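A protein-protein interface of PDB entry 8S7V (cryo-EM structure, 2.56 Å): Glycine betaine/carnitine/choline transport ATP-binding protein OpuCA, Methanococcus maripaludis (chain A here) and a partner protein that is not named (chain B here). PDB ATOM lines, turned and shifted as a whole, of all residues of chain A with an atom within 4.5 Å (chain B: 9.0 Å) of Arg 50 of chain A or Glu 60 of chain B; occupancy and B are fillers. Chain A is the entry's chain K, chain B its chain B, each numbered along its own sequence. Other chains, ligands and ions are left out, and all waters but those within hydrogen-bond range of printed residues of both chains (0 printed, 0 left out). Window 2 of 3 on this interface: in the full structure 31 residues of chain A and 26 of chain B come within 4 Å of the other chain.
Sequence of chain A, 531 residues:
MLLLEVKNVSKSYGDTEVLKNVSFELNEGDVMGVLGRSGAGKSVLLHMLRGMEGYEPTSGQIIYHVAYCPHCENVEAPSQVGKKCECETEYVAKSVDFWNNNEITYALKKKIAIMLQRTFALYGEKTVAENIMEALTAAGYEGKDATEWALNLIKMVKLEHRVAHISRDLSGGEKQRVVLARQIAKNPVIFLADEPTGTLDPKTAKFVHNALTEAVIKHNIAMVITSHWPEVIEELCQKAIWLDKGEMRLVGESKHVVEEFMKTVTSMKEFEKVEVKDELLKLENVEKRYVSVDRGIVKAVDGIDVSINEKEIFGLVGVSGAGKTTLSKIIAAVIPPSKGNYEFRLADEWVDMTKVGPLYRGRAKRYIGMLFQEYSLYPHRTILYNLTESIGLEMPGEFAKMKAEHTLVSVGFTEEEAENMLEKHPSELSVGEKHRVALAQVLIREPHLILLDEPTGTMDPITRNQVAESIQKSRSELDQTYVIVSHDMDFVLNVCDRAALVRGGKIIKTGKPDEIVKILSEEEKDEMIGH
The side-chain carboxylate of Glu 60 of chain B lies within hydrogen-bond range of the backbone NH of Glu 53 of chain A (3.3 Å).
The backbone carbonyl oxygen (O) of His 47 of chain A sits at hydrogen-bond distance from the backbone NH (N) of Met 52 of chain A, at 3.2 Å.
Among the printed residues, pairs that only touch across the chains: Ile 114 of chain A with Glu 61 of chain B (3.2 Å), Met 52 of chain A with Glu 61 of chain B (3.3 Å), Met 52 of chain A with Glu 60 of chain B (3.5 Å) and Arg 50 of chain A with Glu 60 of chain B (3.5 Å).
No residue of chain B comes within 4 Å of Gly 51 of chain A. Of the printed residues of chain B, Met 52 of chain A touches Glu 60 (3.5 Å) and Glu 61 (3.3 Å). Printed residues of chain B within 4 Å of Glu 53 of chain A: Glu 60. Printed residues of chain B within 4 Å of Ile 114 of chain A: Glu 61. Leu 192 of chain A touches none of the printed residues of chain B. Glu 60 of chain B touches just these residues of chain A: Arg 50 (3.5 Å), Met 52 (3.5 Å) and Glu 53 (2.8 Å). Of the printed residues of chain A, Glu 61 of chain B touches Met 52 and Ile 114. The nearest residue of chain B that does not touch Arg 50 of chain A is Glu 61 of chain B (4.1 Å). The nearest printed residue of chain B that does not touch Met 52 of chain A is Pro 58 of chain B (6.1 Å).
Of the 13 printed residues of chain A, 4 touch a printed residue of chain B. Hydrophobic or aromatic side chains of chain A that line the printed part of chain B: Met 52 and Ile 114. Of the 14 printed residues of chain B, 2 touch a printed residue of chain A. Printed residues of chain B that touch a printed residue of chain A: Glu 60 and Glu 61. Among the printed residues, no Asp or Glu carboxylate lies within 4 Å of a Lys or Arg side-chain nitrogen of the other chain.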
ATOM      1  N   LEU A  46      -7.202 -36.561  -6.495  1.00  0.00           N
ATOM      2  CA  LEU A  46      -7.327 -35.173  -6.060  1.00  0.00           C
ATOM      3  C   LEU A  46      -8.700 -34.595  -6.386  1.00  0.00           C
ATOM      4  O   LEU A  46      -9.301 -33.916  -5.547  1.00  0.00           O
ATOM      5  CB  LEU A  46      -6.219 -34.324  -6.677  1.00  0.00           C
ATOM      6  CG  LEU A  46      -5.119 -33.976  -5.673  1.00  0.00           C
ATOM      7  CD1 LEU A  46      -4.502 -35.239  -5.111  1.00  0.00           C
ATOM      8  CD2 LEU A  46      -4.056 -33.101  -6.309  1.00  0.00           C
ATOM      9  N   HIS A  47      -9.214 -34.854  -7.590  1.00  0.00           N
ATOM     10  CA  HIS A  47     -10.572 -34.425  -7.911  1.00  0.00           C
ATOM     11  C   HIS A  47     -11.602 -35.178  -7.080  1.00  0.00           C
ATOM     12  O   HIS A  47     -12.684 -34.651  -6.802  1.00  0.00           O
ATOM     13  CB  HIS A  47     -10.842 -34.615  -9.401  1.00  0.00           C
ATOM     14  CG  HIS A  47      -9.936 -33.814 -10.282  1.00  0.00           C
ATOM     15  ND1 HIS A  47      -9.807 -34.052 -11.633  1.00  0.00           N
ATOM     16  CD2 HIS A  47      -9.115 -32.774 -10.004  1.00  0.00           C
ATOM     17  CE1 HIS A  47      -8.944 -33.196 -12.149  1.00  0.00           C
ATOM     18  NE2 HIS A  47      -8.510 -32.410 -11.181  1.00  0.00           N
ATOM     19  N   MET A  48     -11.280 -36.411  -6.691  1.00  0.00           N
ATOM     20  CA  MET A  48     -12.104 -37.179  -5.767  1.00  0.00           C
ATOM     21  C   MET A  48     -12.232 -36.460  -4.434  1.00  0.00           C
ATOM     22  O   MET A  48     -13.329 -36.335  -3.878  1.00  0.00           O
ATOM     23  CB  MET A  48     -11.454 -38.548  -5.576  1.00  0.00           C
ATOM     24  CG  MET A  48     -12.222 -39.590  -4.815  1.00  0.00           C
ATOM     25  SD  MET A  48     -12.067 -41.132  -5.723  1.00  0.00           S
ATOM     26  CE  MET A  48     -13.458 -42.030  -5.088  1.00  0.00           C
ATOM     27  N   LEU A  49     -11.102 -35.990  -3.905  1.00  0.00           N
ATOM     28  CA  LEU A  49     -11.103 -35.253  -2.646  1.00  0.00           C
ATOM     29  C   LEU A  49     -11.790 -33.901  -2.783  1.00  0.00           C
ATOM     30  O   LEU A  49     -12.494 -33.471  -1.863  1.00  0.00           O
ATOM     31  CB  LEU A  49      -9.671 -35.068  -2.146  1.00  0.00           C
ATOM     32  CG  LEU A  49      -8.882 -36.332  -1.809  1.00  0.00           C
ATOM     33  CD1 LEU A  49      -7.525 -35.970  -1.239  1.00  0.00           C
ATOM     34  CD2 LEU A  49      -9.662 -37.197  -0.835  1.00  0.00           C
ATOM     35  N   ARG A  50     -11.592 -33.218  -3.913  1.00  0.00           N
ATOM     36  CA  ARG A  50     -12.182 -31.895  -4.097  1.00  0.00           C
ATOM     37  C   ARG A  50     -13.698 -31.962  -4.228  1.00  0.00           C
ATOM     38  O   ARG A  50     -14.391 -30.995  -3.892  1.00  0.00           O
ATOM     39  CB  ARG A  50     -11.562 -31.217  -5.321  1.00  0.00           C
ATOM     40  CG  ARG A  50     -12.110 -29.835  -5.634  1.00  0.00           C
ATOM     41  CD  ARG A  50     -11.878 -28.874  -4.481  1.00  0.00           C
ATOM     42  NE  ARG A  50     -12.069 -27.482  -4.867  1.00  0.00           N
ATOM     43  CZ  ARG A  50     -13.243 -26.922  -5.121  1.00  0.00           C
ATOM     44  NH1 ARG A  50     -14.369 -27.611  -5.046  1.00  0.00           N
ATOM     45  NH2 ARG A  50     -13.290 -25.637  -5.459  1.00  0.00           N
ATOM     46  N   GLY A  51     -14.232 -33.087  -4.692  1.00  0.00           N
ATOM     47  CA  GLY A  51     -15.666 -33.213  -4.851  1.00  0.00           C
ATOM     48  C   GLY A  51     -16.191 -32.828  -6.214  1.00  0.00           C
ATOM     49  O   GLY A  51     -17.368 -32.475  -6.339  1.00  0.00           O
ATOM     50  N   MET A  52     -15.352 -32.885  -7.243  1.00  0.00           N
ATOM     51  CA  MET A  52     -15.781 -32.553  -8.590  1.00  0.00           C
ATOM     52  C   MET A  52     -16.746 -33.611  -9.119  1.00  0.00           C
ATOM     53  O   MET A  52     -16.727 -34.771  -8.705  1.00  0.00           O
ATOM     54  CB  MET A  52     -14.573 -32.425  -9.518  1.00  0.00           C
ATOM     55  CG  MET A  52     -13.709 -31.209  -9.237  1.00  0.00           C
ATOM     56  SD  MET A  52     -12.364 -31.013 -10.419  1.00  0.00           S
ATOM     57  CE  MET A  52     -12.421 -29.248 -10.705  1.00  0.00           C
ATOM     58  N   GLU A  53     -17.600 -33.190 -10.048  1.00  0.00           N
ATOM     59  CA  GLU A  53     -18.639 -34.073 -10.561  1.00  0.00           C
ATOM     60  C   GLU A  53     -18.027 -35.214 -11.366  1.00  0.00           C
ATOM     61  O   GLU A  53     -17.025 -35.039 -12.064  1.00  0.00           O
ATOM     62  CB  GLU A  53     -19.632 -33.284 -11.418  1.00  0.00           C
ATOM     63  CG  GLU A  53     -19.205 -32.972 -12.860  1.00  0.00           C
ATOM     64  CD  GLU A  53     -18.013 -32.029 -12.984  1.00  0.00           C
ATOM     65  OE1 GLU A  53     -17.113 -32.039 -12.119  1.00  0.00           O
ATOM     66  OE2 GLU A  53     -17.977 -31.260 -13.968  1.00  0.00           O
ATOM     67  N   PHE A  98     -18.393 -37.146   2.573  1.00  0.00           N
ATOM     68  CA  PHE A  98     -18.517 -36.588   1.233  1.00  0.00           C
ATOM     69  C   PHE A  98     -19.394 -37.479   0.360  1.00  0.00           C
ATOM     70  O   PHE A  98     -19.460 -38.697   0.546  1.00  0.00           O
ATOM     71  CB  PHE A  98     -17.140 -36.416   0.596  1.00  0.00           C
ATOM     72  CG  PHE A  98     -16.805 -34.994   0.254  1.00  0.00           C
ATOM     73  CD1 PHE A  98     -17.412 -33.945   0.922  1.00  0.00           C
ATOM     74  CD2 PHE A  98     -15.883 -34.704  -0.736  1.00  0.00           C
ATOM     75  CE1 PHE A  98     -17.107 -32.637   0.608  1.00  0.00           C
ATOM     76  CE2 PHE A  98     -15.574 -33.398  -1.054  1.00  0.00           C
ATOM     77  CZ  PHE A  98     -16.187 -32.364  -0.380  1.00  0.00           C
ATOM     78  N   LYS A 109     -17.161 -27.216   0.692  1.00  0.00           N
ATOM     79  CA  LYS A 109     -16.496 -27.181  -0.604  1.00  0.00           C
ATOM     80  C   LYS A 109     -15.926 -25.800  -0.909  1.00  0.00           C
ATOM     81  O   LYS A 109     -14.971 -25.683  -1.684  1.00  0.00           O
ATOM     82  CB  LYS A 109     -17.475 -27.631  -1.691  1.00  0.00           C
ATOM     83  CG  LYS A 109     -16.982 -27.501  -3.118  1.00  0.00           C
ATOM     84  CD  LYS A 109     -17.855 -28.298  -4.079  1.00  0.00           C
ATOM     85  CE  LYS A 109     -18.421 -29.548  -3.418  1.00  0.00           C
ATOM     86  NZ  LYS A 109     -18.792 -30.593  -4.411  1.00  0.00           N
ATOM     87  N   ILE A 112     -12.171 -25.550   0.630  1.00  0.00           N
ATOM     88  CA  ILE A 112     -11.120 -26.420   0.118  1.00  0.00           C
ATOM     89  C   ILE A 112     -10.607 -25.838  -1.191  1.00  0.00           C
ATOM     90  O   ILE A 112     -11.391 -25.441  -2.060  1.00  0.00           O
ATOM     91  CB  ILE A 112     -11.604 -27.876  -0.062  1.00  0.00           C
ATOM     92  CG1 ILE A 112     -12.740 -27.969  -1.081  1.00  0.00           C
ATOM     93  CG2 ILE A 112     -12.069 -28.444   1.269  1.00  0.00           C
ATOM     94  CD1 ILE A 112     -13.512 -29.270  -1.012  1.00  0.00           C
ATOM     95  N   ILE A 114      -8.024 -26.126  -4.604  1.00  0.00           N
ATOM     96  CA  ILE A 114      -7.412 -27.095  -5.505  1.00  0.00           C
ATOM     97  C   ILE A 114      -6.623 -26.347  -6.570  1.00  0.00           C
ATOM     98  O   ILE A 114      -7.096 -25.343  -7.113  1.00  0.00           O
ATOM     99  CB  ILE A 114      -8.458 -28.025  -6.154  1.00  0.00           C
ATOM    100  CG1 ILE A 114      -7.788 -28.980  -7.144  1.00  0.00           C
ATOM    101  CG2 ILE A 114      -9.540 -27.221  -6.850  1.00  0.00           C
ATOM    102  CD1 ILE A 114      -8.348 -30.381  -7.110  1.00  0.00           C
ATOM    103  N   LEU A 192      -5.214 -28.876  -1.961  1.00  0.00           N
ATOM    104  CA  LEU A 192      -4.920 -29.941  -2.912  1.00  0.00           C
ATOM    105  C   LEU A 192      -4.151 -29.340  -4.083  1.00  0.00           C
ATOM    106  O   LEU A 192      -4.708 -28.567  -4.868  1.00  0.00           O
ATOM    107  CB  LEU A 192      -6.209 -30.610  -3.383  1.00  0.00           C
ATOM    108  CG  LEU A 192      -7.191 -31.010  -2.283  1.00  0.00           C
ATOM    109  CD1 LEU A 192      -8.602 -31.099  -2.834  1.00  0.00           C
ATOM    110  CD2 LEU A 192      -6.775 -32.324  -1.649  1.00  0.00           C
ATOM    111  N   HIS B  56     -13.458 -16.600 -17.487  1.00  0.00           N
ATOM    112  CA  HIS B  56     -13.569 -16.774 -16.047  1.00  0.00           C
ATOM    113  C   HIS B  56     -13.026 -18.149 -15.694  1.00  0.00           C
ATOM    114  O   HIS B  56     -12.900 -19.013 -16.569  1.00  0.00           O
ATOM    115  CB  HIS B  56     -15.020 -16.623 -15.573  1.00  0.00           C
ATOM    116  CG  HIS B  56     -15.988 -17.523 -16.275  1.00  0.00           C
ATOM    117  ND1 HIS B  56     -16.135 -18.855 -15.951  1.00  0.00           N
ATOM    118  CD2 HIS B  56     -16.865 -17.280 -17.277  1.00  0.00           C
ATOM    119  CE1 HIS B  56     -17.058 -19.394 -16.727  1.00  0.00           C
ATOM    120  NE2 HIS B  56     -17.516 -18.459 -17.540  1.00  0.00           N
ATOM    121  N   PRO B  57     -12.668 -18.375 -14.433  1.00  0.00           N
ATOM    122  CA  PRO B  57     -12.227 -19.713 -14.006  1.00  0.00           C
ATOM    123  C   PRO B  57     -13.286 -20.761 -14.300  1.00  0.00           C
ATOM    124  O   PRO B  57     -14.449 -20.422 -14.572  1.00  0.00           O
ATOM    125  CB  PRO B  57     -12.012 -19.560 -12.493  1.00  0.00           C
ATOM    126  CG  PRO B  57     -12.075 -18.112 -12.193  1.00  0.00           C
ATOM    127  CD  PRO B  57     -12.385 -17.339 -13.427  1.00  0.00           C
ATOM    128  N   PRO B  58     -12.928 -22.044 -14.258  1.00  0.00           N
ATOM    129  CA  PRO B  58     -13.935 -23.091 -14.449  1.00  0.00           C
ATOM    130  C   PRO B  58     -15.033 -22.991 -13.403  1.00  0.00           C
ATOM    131  O   PRO B  58     -14.815 -22.514 -12.288  1.00  0.00           O
ATOM    132  CB  PRO B  58     -13.133 -24.388 -14.297  1.00  0.00           C
ATOM    133  CG  PRO B  58     -11.746 -24.009 -14.658  1.00  0.00           C
ATOM    134  CD  PRO B  58     -11.567 -22.598 -14.181  1.00  0.00           C
ATOM    135  N   LEU B  59     -16.232 -23.438 -13.784  1.00  0.00           N
ATOM    136  CA  LEU B  59     -17.394 -23.284 -12.915  1.00  0.00           C
ATOM    137  C   LEU B  59     -17.205 -23.983 -11.576  1.00  0.00           C
ATOM    138  O   LEU B  59     -17.825 -23.592 -10.582  1.00  0.00           O
ATOM    139  CB  LEU B  59     -18.647 -23.811 -13.613  1.00  0.00           C
ATOM    140  CG  LEU B  59     -19.095 -23.059 -14.866  1.00  0.00           C
ATOM    141  CD1 LEU B  59     -20.438 -23.581 -15.340  1.00  0.00           C
ATOM    142  CD2 LEU B  59     -19.159 -21.566 -14.601  1.00  0.00           C
ATOM    143  N   GLU B  60     -16.364 -25.017 -11.526  1.00  0.00           N
ATOM    144  CA  GLU B  60     -16.093 -25.676 -10.253  1.00  0.00           C
ATOM    145  C   GLU B  60     -15.248 -24.794  -9.344  1.00  0.00           C
ATOM    146  O   GLU B  60     -15.443 -24.787  -8.122  1.00  0.00           O
ATOM    147  CB  GLU B  60     -15.405 -27.018 -10.490  1.00  0.00           C
ATOM    148  CG  GLU B  60     -16.182 -27.964 -11.384  1.00  0.00           C
ATOM    149  CD  GLU B  60     -17.279 -28.695 -10.638  1.00  0.00           C
ATOM    150  OE1 GLU B  60     -18.298 -28.058 -10.302  1.00  0.00           O
ATOM    151  OE2 GLU B  60     -17.118 -29.904 -10.379  1.00  0.00           O
ATOM    152  N   GLU B  61     -14.304 -24.048  -9.916  1.00  0.00           N
ATOM    153  CA  GLU B  61     -13.451 -23.187  -9.103  1.00  0.00           C
ATOM    154  C   GLU B  61     -14.234 -22.021  -8.514  1.00  0.00           C
ATOM    155  O   GLU B  61     -14.109 -21.729  -7.319  1.00  0.00           O
ATOM    156  CB  GLU B  61     -12.275 -22.682  -9.937  1.00  0.00           C
ATOM    157  CG  GLU B  61     -11.492 -23.784 -10.629  1.00  0.00           C
ATOM    158  CD  GLU B  61     -11.236 -24.975  -9.727  1.00  0.00           C
ATOM    159  OE1 GLU B  61     -10.793 -24.770  -8.577  1.00  0.00           O
ATOM    160  OE2 GLU B  61     -11.482 -26.118 -10.164  1.00  0.00           O
ATOM    161  N   MET B  62     -15.039 -21.344  -9.327  1.00  0.00           N
ATOM    162  CA  MET B  62     -15.803 -20.209  -8.830  1.00  0.00           C
ATOM    163  C   MET B  62     -16.912 -20.685  -7.902  1.00  0.00           C
ATOM    164  O   MET B  62     -17.432 -21.796  -8.046  1.00  0.00           O
ATOM    165  CB  MET B  62     -16.390 -19.404  -9.988  1.00  0.00           C
ATOM    166  CG  MET B  62     -15.518 -19.373 -11.229  1.00  0.00           C
ATOM    167  SD  MET B  62     -16.334 -18.628 -12.652  1.00  0.00           S
ATOM    168  CE  MET B  62     -17.362 -17.403 -11.852  1.00  0.00           C
ATOM    169  N   ASP B  63     -17.265 -19.842  -6.938  1.00  0.00           N
ATOM    170  CA  ASP B  63     -18.290 -20.160  -5.953  1.00  0.00           C
ATOM    171  C   ASP B  63     -19.554 -19.371  -6.269  1.00  0.00           C
ATOM    172  O   ASP B  63     -19.500 -18.147  -6.433  1.00  0.00           O
ATOM    173  CB  ASP B  63     -17.801 -19.850  -4.540  1.00  0.00           C
ATOM    174  CG  ASP B  63     -16.731 -20.816  -4.071  1.00  0.00           C
ATOM    175  OD1 ASP B  63     -16.912 -22.038  -4.250  1.00  0.00           O
ATOM    176  OD2 ASP B  63     -15.709 -20.352  -3.523  1.00  0.00           O
ATOM    177  N   PHE B  64     -20.678 -20.069  -6.357  1.00  0.00           N
ATOM    178  CA  PHE B  64     -21.981 -19.461  -6.573  1.00  0.00           C
ATOM    179  C   PHE B  64     -22.906 -19.803  -5.417  1.00  0.00           C
ATOM    180  O   PHE B  64     -22.742 -20.817  -4.734  1.00  0.00           O
ATOM    181  CB  PHE B  64     -22.598 -19.933  -7.894  1.00  0.00           C
ATOM    182  CG  PHE B  64     -21.696 -19.770  -9.078  1.00  0.00           C
ATOM    183  CD1 PHE B  64     -21.511 -18.531  -9.660  1.00  0.00           C
ATOM    184  CD2 PHE B  64     -21.041 -20.862  -9.617  1.00  0.00           C
ATOM    185  CE1 PHE B  64     -20.685 -18.382 -10.752  1.00  0.00           C
ATOM    186  CE2 PHE B  64     -20.214 -20.720 -10.708  1.00  0.00           C
ATOM    187  CZ  PHE B  64     -20.037 -19.480 -11.276  1.00  0.00           C
ATOM    188  N   PRO B  75     -24.786 -27.190 -18.007  1.00  0.00           N
ATOM    189  CA  PRO B  75     -24.069 -26.197 -18.810  1.00  0.00           C
ATOM    190  C   PRO B  75     -23.290 -26.834 -19.952  1.00  0.00           C
ATOM    191  O   PRO B  75     -23.019 -28.035 -19.973  1.00  0.00           O
ATOM    192  CB  PRO B  75     -23.120 -25.550 -17.797  1.00  0.00           C
ATOM    193  CG  PRO B  75     -22.860 -26.623 -16.810  1.00  0.00           C
ATOM    194  CD  PRO B  75     -24.114 -27.451 -16.723  1.00  0.00           C
ATOM    195  N   ALA B  79     -18.760 -23.530 -21.345  1.00  0.00           N
ATOM    196  CA  ALA B  79     -19.088 -22.842 -20.103  1.00  0.00           C
ATOM    197  C   ALA B  79     -18.449 -23.514 -18.897  1.00  0.00           C
ATOM    198  O   ALA B  79     -17.991 -22.825 -17.980  1.00  0.00           O
ATOM    199  CB  ALA B  79     -20.604 -22.777 -19.920  1.00  0.00           C
ATOM    200  N   LYS B  80     -18.413 -24.848 -18.881  1.00  0.00           N
ATOM    201  CA  LYS B  80     -17.835 -25.568 -17.751  1.00  0.00           C
ATOM    202  C   LYS B  80     -16.362 -25.227 -17.578  1.00  0.00           C
ATOM    203  O   LYS B  80     -15.905 -24.948 -16.464  1.00  0.00           O
ATOM    204  CB  LYS B  80     -18.018 -27.071 -17.945  1.00  0.00           C
ATOM    205  CG  LYS B  80     -19.112 -27.678 -17.093  1.00  0.00           C
ATOM    206  CD  LYS B  80     -19.199 -29.176 -17.306  1.00  0.00           C
ATOM    207  CE  LYS B  80     -20.422 -29.541 -18.127  1.00  0.00           C
ATOM    208  NZ  LYS B  80     -20.839 -30.953 -17.903  1.00  0.00           N
ATOM    209  N   GLU B  81     -15.670 -25.036 -18.704  1.00  0.00           N
ATOM    210  CA  GLU B  81     -14.229 -24.665 -18.664  1.00  0.00           C
ATOM    211  C   GLU B  81     -14.064 -23.147 -18.524  1.00  0.00           C
ATOM    212  O   GLU B  81     -13.128 -22.729 -17.828  1.00  0.00           O
ATOM    213  CB  GLU B  81     -13.523 -25.162 -19.925  1.00  0.00           C
ATOM    214  CG  GLU B  81     -13.744 -26.634 -20.217  1.00  0.00           C
ATOM    215  CD  GLU B  81     -13.718 -27.550 -19.007  1.00  0.00           C
ATOM    216  OE1 GLU B  81     -12.671 -27.607 -18.332  1.00  0.00           O
ATOM    217  OE2 GLU B  81     -14.744 -28.209 -18.746  1.00  0.00           O
ATOM    218  N   GLY B  82     -14.915 -22.353 -19.180  1.00  0.00           N
ATOM    219  CA  GLY B  82     -14.862 -20.884 -19.036  1.00  0.00           C
ATOM    220  C   GLY B  82     -14.312 -20.198 -20.271  1.00  0.00           C
ATOM    221  O   GLY B  82     -13.515 -19.274 -20.099  1.00  0.00           O
